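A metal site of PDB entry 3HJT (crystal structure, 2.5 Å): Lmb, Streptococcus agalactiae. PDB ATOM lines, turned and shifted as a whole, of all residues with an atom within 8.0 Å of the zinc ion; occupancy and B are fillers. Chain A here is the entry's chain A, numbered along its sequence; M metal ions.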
ATOM      1  N   PHE A  20      -2.839  22.036  29.816  1.00  0.00           N
ATOM      2  CA  PHE A  20      -3.580  21.887  28.563  1.00  0.00           C
ATOM      3  C   PHE A  20      -4.886  21.125  28.812  1.00  0.00           C
ATOM      4  O   PHE A  20      -5.258  20.916  29.971  1.00  0.00           O
ATOM      5  CB  PHE A  20      -2.724  21.244  27.449  1.00  0.00           C
ATOM      6  CG  PHE A  20      -2.303  19.832  27.721  1.00  0.00           C
ATOM      7  CD1 PHE A  20      -1.723  19.493  28.937  1.00  0.00           C
ATOM      8  CD2 PHE A  20      -2.433  18.864  26.739  1.00  0.00           C
ATOM      9  CE1 PHE A  20      -1.280  18.196  29.160  1.00  0.00           C
ATOM     10  CE2 PHE A  20      -2.004  17.570  26.954  1.00  0.00           C
ATOM     11  CZ  PHE A  20      -1.426  17.231  28.159  1.00  0.00           C
ATOM     12  N   ILE A  46       1.084  21.872  22.562  1.00  0.00           N
ATOM     13  CA  ILE A  46       1.453  21.691  23.962  1.00  0.00           C
ATOM     14  C   ILE A  46       2.861  21.139  24.064  1.00  0.00           C
ATOM     15  O   ILE A  46       3.553  21.320  25.079  1.00  0.00           O
ATOM     16  CB  ILE A  46       0.522  20.699  24.688  1.00  0.00           C
ATOM     17  CG1 ILE A  46       0.949  20.549  26.141  1.00  0.00           C
ATOM     18  CG2 ILE A  46       0.572  19.349  23.999  1.00  0.00           C
ATOM     19  CD1 ILE A  46       0.928  21.845  26.910  1.00  0.00           C
ATOM     20  N   HIS A  47       3.265  20.454  23.000  1.00  0.00           N
ATOM     21  CA  HIS A  47       4.597  19.872  22.930  1.00  0.00           C
ATOM     22  C   HIS A  47       5.689  20.927  22.799  1.00  0.00           C
ATOM     23  O   HIS A  47       6.693  20.904  23.510  1.00  0.00           O
ATOM     24  CB  HIS A  47       4.664  18.934  21.745  1.00  0.00           C
ATOM     25  CG  HIS A  47       4.188  17.554  22.050  1.00  0.00           C
ATOM     26  ND1 HIS A  47       4.929  16.657  22.794  1.00  0.00           N
ATOM     27  CD2 HIS A  47       3.042  16.905  21.732  1.00  0.00           C
ATOM     28  CE1 HIS A  47       4.270  15.520  22.904  1.00  0.00           C
ATOM     29  NE2 HIS A  47       3.113  15.653  22.274  1.00  0.00           N
ATOM     30  N   LEU A  72       6.699  16.784  29.528  1.00  0.00           N
ATOM     31  CA  LEU A  72       5.860  17.469  28.563  1.00  0.00           C
ATOM     32  C   LEU A  72       6.005  18.950  28.842  1.00  0.00           C
ATOM     33  O   LEU A  72       6.738  19.640  28.144  1.00  0.00           O
ATOM     34  CB  LEU A  72       4.402  17.035  28.670  1.00  0.00           C
ATOM     35  CG  LEU A  72       3.438  17.493  27.560  1.00  0.00           C
ATOM     36  CD1 LEU A  72       4.001  17.135  26.200  1.00  0.00           C
ATOM     37  CD2 LEU A  72       2.070  16.845  27.729  1.00  0.00           C
ATOM     38  N   ASP A 121       7.705   8.739  27.009  1.00  0.00           N
ATOM     39  CA  ASP A 121       6.450   8.990  26.303  1.00  0.00           C
ATOM     40  C   ASP A 121       5.447   9.507  27.348  1.00  0.00           C
ATOM     41  O   ASP A 121       5.034   8.763  28.247  1.00  0.00           O
ATOM     42  CB  ASP A 121       5.955   7.672  25.700  1.00  0.00           C
ATOM     43  CG  ASP A 121       4.897   7.874  24.643  1.00  0.00           C
ATOM     44  OD1 ASP A 121       4.034   8.756  24.809  1.00  0.00           O
ATOM     45  OD2 ASP A 121       4.925   7.118  23.654  1.00  0.00           O
ATOM     46  N   PRO A 122       5.072  10.796  27.259  1.00  0.00           N
ATOM     47  CA  PRO A 122       4.134  11.383  28.224  1.00  0.00           C
ATOM     48  C   PRO A 122       2.640  11.056  27.996  1.00  0.00           C
ATOM     49  O   PRO A 122       1.811  11.259  28.889  1.00  0.00           O
ATOM     50  CB  PRO A 122       4.455  12.882  28.100  1.00  0.00           C
ATOM     51  CG  PRO A 122       4.702  13.025  26.596  1.00  0.00           C
ATOM     52  CD  PRO A 122       5.509  11.781  26.244  1.00  0.00           C
ATOM     53  N   HIS A 123       2.314  10.541  26.809  1.00  0.00           N
ATOM     54  CA  HIS A 123       0.936  10.210  26.399  1.00  0.00           C
ATOM     55  C   HIS A 123       0.087   9.205  27.177  1.00  0.00           C
ATOM     56  O   HIS A 123      -0.623   8.386  26.580  1.00  0.00           O
ATOM     57  CB  HIS A 123       0.959   9.785  24.929  1.00  0.00           C
ATOM     58  CG  HIS A 123       1.572  10.810  24.024  1.00  0.00           C
ATOM     59  ND1 HIS A 123       2.722  10.565  23.291  1.00  0.00           N
ATOM     60  CD2 HIS A 123       1.223  12.091  23.751  1.00  0.00           C
ATOM     61  CE1 HIS A 123       3.047  11.648  22.615  1.00  0.00           C
ATOM     62  NE2 HIS A 123       2.155  12.583  22.871  1.00  0.00           N
ATOM     63  N   TRP A 125      -2.497   9.854  29.299  1.00  0.00           N
ATOM     64  CA  TRP A 125      -3.911  10.243  29.337  1.00  0.00           C
ATOM     65  C   TRP A 125      -4.855   9.651  28.280  1.00  0.00           C
ATOM     66  O   TRP A 125      -6.066   9.762  28.443  1.00  0.00           O
ATOM     67  CB  TRP A 125      -4.025  11.777  29.369  1.00  0.00           C
ATOM     68  CG  TRP A 125      -3.595  12.440  28.100  1.00  0.00           C
ATOM     69  CD1 TRP A 125      -4.334  12.565  26.963  1.00  0.00           C
ATOM     70  CD2 TRP A 125      -2.300  12.980  27.803  1.00  0.00           C
ATOM     71  NE1 TRP A 125      -3.580  13.143  25.966  1.00  0.00           N
ATOM     72  CE2 TRP A 125      -2.325  13.406  26.464  1.00  0.00           C
ATOM     73  CE3 TRP A 125      -1.120  13.144  28.535  1.00  0.00           C
ATOM     74  CZ2 TRP A 125      -1.216  13.994  25.832  1.00  0.00           C
ATOM     75  CZ3 TRP A 125      -0.006  13.723  27.913  1.00  0.00           C
ATOM     76  CH2 TRP A 125      -0.071  14.139  26.569  1.00  0.00           C
ATOM     77  N   HIS A 187       1.143  11.407  14.763  1.00  0.00           N
ATOM     78  CA  HIS A 187       2.367  11.333  15.534  1.00  0.00           C
ATOM     79  C   HIS A 187       2.220  10.300  16.631  1.00  0.00           C
ATOM     80  O   HIS A 187       1.131   9.748  16.867  1.00  0.00           O
ATOM     81  CB  HIS A 187       2.803  12.720  16.059  1.00  0.00           C
ATOM     82  CG  HIS A 187       2.106  13.188  17.306  1.00  0.00           C
ATOM     83  ND1 HIS A 187       0.869  13.787  17.294  1.00  0.00           N
ATOM     84  CD2 HIS A 187       2.548  13.264  18.594  1.00  0.00           C
ATOM     85  CE1 HIS A 187       0.572  14.211  18.522  1.00  0.00           C
ATOM     86  NE2 HIS A 187       1.573  13.901  19.318  1.00  0.00           N
ATOM     87  N   THR A 188       3.332  10.005  17.285  1.00  0.00           N
ATOM     88  CA  THR A 188       3.349   8.995  18.323  1.00  0.00           C
ATOM     89  C   THR A 188       2.680   9.420  19.610  1.00  0.00           C
ATOM     90  O   THR A 188       3.338   9.764  20.600  1.00  0.00           O
ATOM     91  CB  THR A 188       4.777   8.567  18.577  1.00  0.00           C
ATOM     92  OG1 THR A 188       5.318   8.037  17.360  1.00  0.00           O
ATOM     93  CG2 THR A 188       4.841   7.502  19.654  1.00  0.00           C
ATOM     94  N   ALA A 189       1.353   9.366  19.592  1.00  0.00           N
ATOM     95  CA  ALA A 189       0.578   9.768  20.761  1.00  0.00           C
ATOM     96  C   ALA A 189      -0.354   8.696  21.329  1.00  0.00           C
ATOM     97  O   ALA A 189      -1.000   8.930  22.342  1.00  0.00           O
ATOM     98  CB  ALA A 189      -0.227  11.027  20.427  1.00  0.00           C
ATOM     99  N   PHE A 190      -0.416   7.525  20.703  1.00  0.00           N
ATOM    100  CA  PHE A 190      -1.341   6.514  21.228  1.00  0.00           C
ATOM    101  C   PHE A 190      -0.701   5.209  21.692  1.00  0.00           C
ATOM    102  O   PHE A 190      -1.335   4.155  21.644  1.00  0.00           O
ATOM    103  CB  PHE A 190      -2.444   6.234  20.181  1.00  0.00           C
ATOM    104  CG  PHE A 190      -3.196   7.477  19.741  1.00  0.00           C
ATOM    105  CD1 PHE A 190      -2.745   8.231  18.657  1.00  0.00           C
ATOM    106  CD2 PHE A 190      -4.300   7.929  20.459  1.00  0.00           C
ATOM    107  CE1 PHE A 190      -3.402   9.424  18.300  1.00  0.00           C
ATOM    108  CE2 PHE A 190      -4.952   9.113  20.102  1.00  0.00           C
ATOM    109  CZ  PHE A 190      -4.496   9.859  19.027  1.00  0.00           C
ATOM    110  N   GLY A 206       7.310  11.623  15.468  1.00  0.00           N
ATOM    111  CA  GLY A 206       7.610  11.109  16.793  1.00  0.00           C
ATOM    112  C   GLY A 206       6.702  11.517  17.935  1.00  0.00           C
ATOM    113  O   GLY A 206       5.541  11.909  17.735  1.00  0.00           O
ATOM    114  N   ILE A 207       7.238  11.406  19.153  1.00  0.00           N
ATOM    115  CA  ILE A 207       6.509  11.754  20.360  1.00  0.00           C
ATOM    116  C   ILE A 207       5.925  13.167  20.246  1.00  0.00           C
ATOM    117  O   ILE A 207       4.865  13.439  20.817  1.00  0.00           O
ATOM    118  CB  ILE A 207       7.451  11.682  21.603  1.00  0.00           C
ATOM    119  CG1 ILE A 207       7.806  10.233  21.914  1.00  0.00           C
ATOM    120  CG2 ILE A 207       6.777  12.310  22.819  1.00  0.00           C
ATOM    121  CD1 ILE A 207       6.679   9.442  22.519  1.00  0.00           C
ATOM    122  N   SER A 208       6.612  14.038  19.512  1.00  0.00           N
ATOM    123  CA  SER A 208       6.178  15.420  19.274  1.00  0.00           C
ATOM    124  C   SER A 208       5.860  15.595  17.798  1.00  0.00           C
ATOM    125  O   SER A 208       6.518  15.002  16.944  1.00  0.00           O
ATOM    126  CB  SER A 208       7.285  16.424  19.647  1.00  0.00           C
ATOM    127  OG  SER A 208       6.954  17.738  19.209  1.00  0.00           O
ATOM    128  N   PRO A 209       4.851  16.412  17.478  1.00  0.00           N
ATOM    129  CA  PRO A 209       4.516  16.612  16.063  1.00  0.00           C
ATOM    130  C   PRO A 209       5.656  17.297  15.292  1.00  0.00           C
ATOM    131  O   PRO A 209       5.657  17.327  14.062  1.00  0.00           O
ATOM    132  CB  PRO A 209       3.247  17.456  16.133  1.00  0.00           C
ATOM    133  CG  PRO A 209       2.650  17.065  17.435  1.00  0.00           C
ATOM    134  CD  PRO A 209       3.847  17.033  18.347  1.00  0.00           C
ATOM    135  N   GLU A 236      -4.708  14.393  12.475  1.00  0.00           N
ATOM    136  CA  GLU A 236      -5.199  15.041  13.691  1.00  0.00           C
ATOM    137  C   GLU A 236      -5.353  16.510  13.327  1.00  0.00           C
ATOM    138  O   GLU A 236      -4.666  17.004  12.423  1.00  0.00           O
ATOM    139  CB  GLU A 236      -4.233  14.869  14.867  1.00  0.00           C
ATOM    140  CG  GLU A 236      -2.861  15.451  14.640  1.00  0.00           C
ATOM    141  CD  GLU A 236      -1.962  15.287  15.863  1.00  0.00           C
ATOM    142  OE1 GLU A 236      -2.197  15.986  16.878  1.00  0.00           O
ATOM    143  OE2 GLU A 236      -1.018  14.471  15.796  1.00  0.00           O
ATOM    144  N   PRO A 260      -5.447  13.062  19.885  1.00  0.00           N
ATOM    145  CA  PRO A 260      -4.739  12.657  21.110  1.00  0.00           C
ATOM    146  C   PRO A 260      -5.201  13.504  22.312  1.00  0.00           C
ATOM    147  O   PRO A 260      -4.591  13.491  23.376  1.00  0.00           O
ATOM    148  CB  PRO A 260      -3.268  12.906  20.760  1.00  0.00           C
ATOM    149  CG  PRO A 260      -3.342  14.067  19.830  1.00  0.00           C
ATOM    150  CD  PRO A 260      -4.536  13.748  18.956  1.00  0.00           C
ATOM    151  N   LEU A 261      -6.292  14.230  22.117  1.00  0.00           N
ATOM    152  CA  LEU A 261      -6.892  15.094  23.142  1.00  0.00           C
ATOM    153  C   LEU A 261      -5.954  16.141  23.702  1.00  0.00           C
ATOM    154  O   LEU A 261      -6.096  16.536  24.854  1.00  0.00           O
ATOM    155  CB  LEU A 261      -7.482  14.252  24.276  1.00  0.00           C
ATOM    156  CG  LEU A 261      -8.685  13.378  23.896  1.00  0.00           C
ATOM    157  CD1 LEU A 261      -9.004  12.411  25.009  1.00  0.00           C
ATOM    158  CD2 LEU A 261      -9.863  14.262  23.612  1.00  0.00           C
ATOM    159  N   GLU A 262      -5.014  16.591  22.884  1.00  0.00           N
ATOM    160  CA  GLU A 262      -4.046  17.610  23.301  1.00  0.00           C
ATOM    161  C   GLU A 262      -4.566  19.025  23.080  1.00  0.00           C
ATOM    162  O   GLU A 262      -3.948  19.977  23.528  1.00  0.00           O
ATOM    163  CB  GLU A 262      -2.736  17.442  22.547  1.00  0.00           C
ATOM    164  CG  GLU A 262      -2.217  16.027  22.597  1.00  0.00           C
ATOM    165  CD  GLU A 262      -0.786  15.935  22.189  1.00  0.00           C
ATOM    166  OE1 GLU A 262      -0.336  16.812  21.430  1.00  0.00           O
ATOM    167  OE2 GLU A 262      -0.108  14.970  22.611  1.00  0.00           O
HETATM  168 ZN    ZN M   1       1.635  14.357  21.462  1.00  0.00          ZN
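ND1 of His 123 lies close to O of Thr 188 (2.9 Å). A ring nitrogen (NE2) of His 47 lies close to the backbone carbonyl oxygen (O) of Ile 207 (3.2 Å). A ring nitrogen (ND1) of His 123 is in hydrogen-bond range of the side-chain carboxylate (OD1) of Asp 121 (2.7 Å). A ring nitrogen (ND1) of His 187 is in hydrogen-bond range of the side-chain carboxylate (OE2) of Glu 236.
Ala 189 touches the zinc ion (CB to ZN, 3.95 Å). Ile 207 touches the zinc ion. Six residues have an atom within 4 Å of the zinc ion: His 47, His 123, His 187, Ala 189, Ile 207 and Glu 262. The nearest printed residue that does not touch the zinc ion is Pro 209 (4.7 Å).
NE2 of His 47 binds the zinc ion. OE2 of Glu 262 binds the zinc ion (2.2 Å). A ring nitrogen (NE2) of His 187 is bound to the zinc ion. The zinc ion is bound by NE2 of His 123 (2.3 Å).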
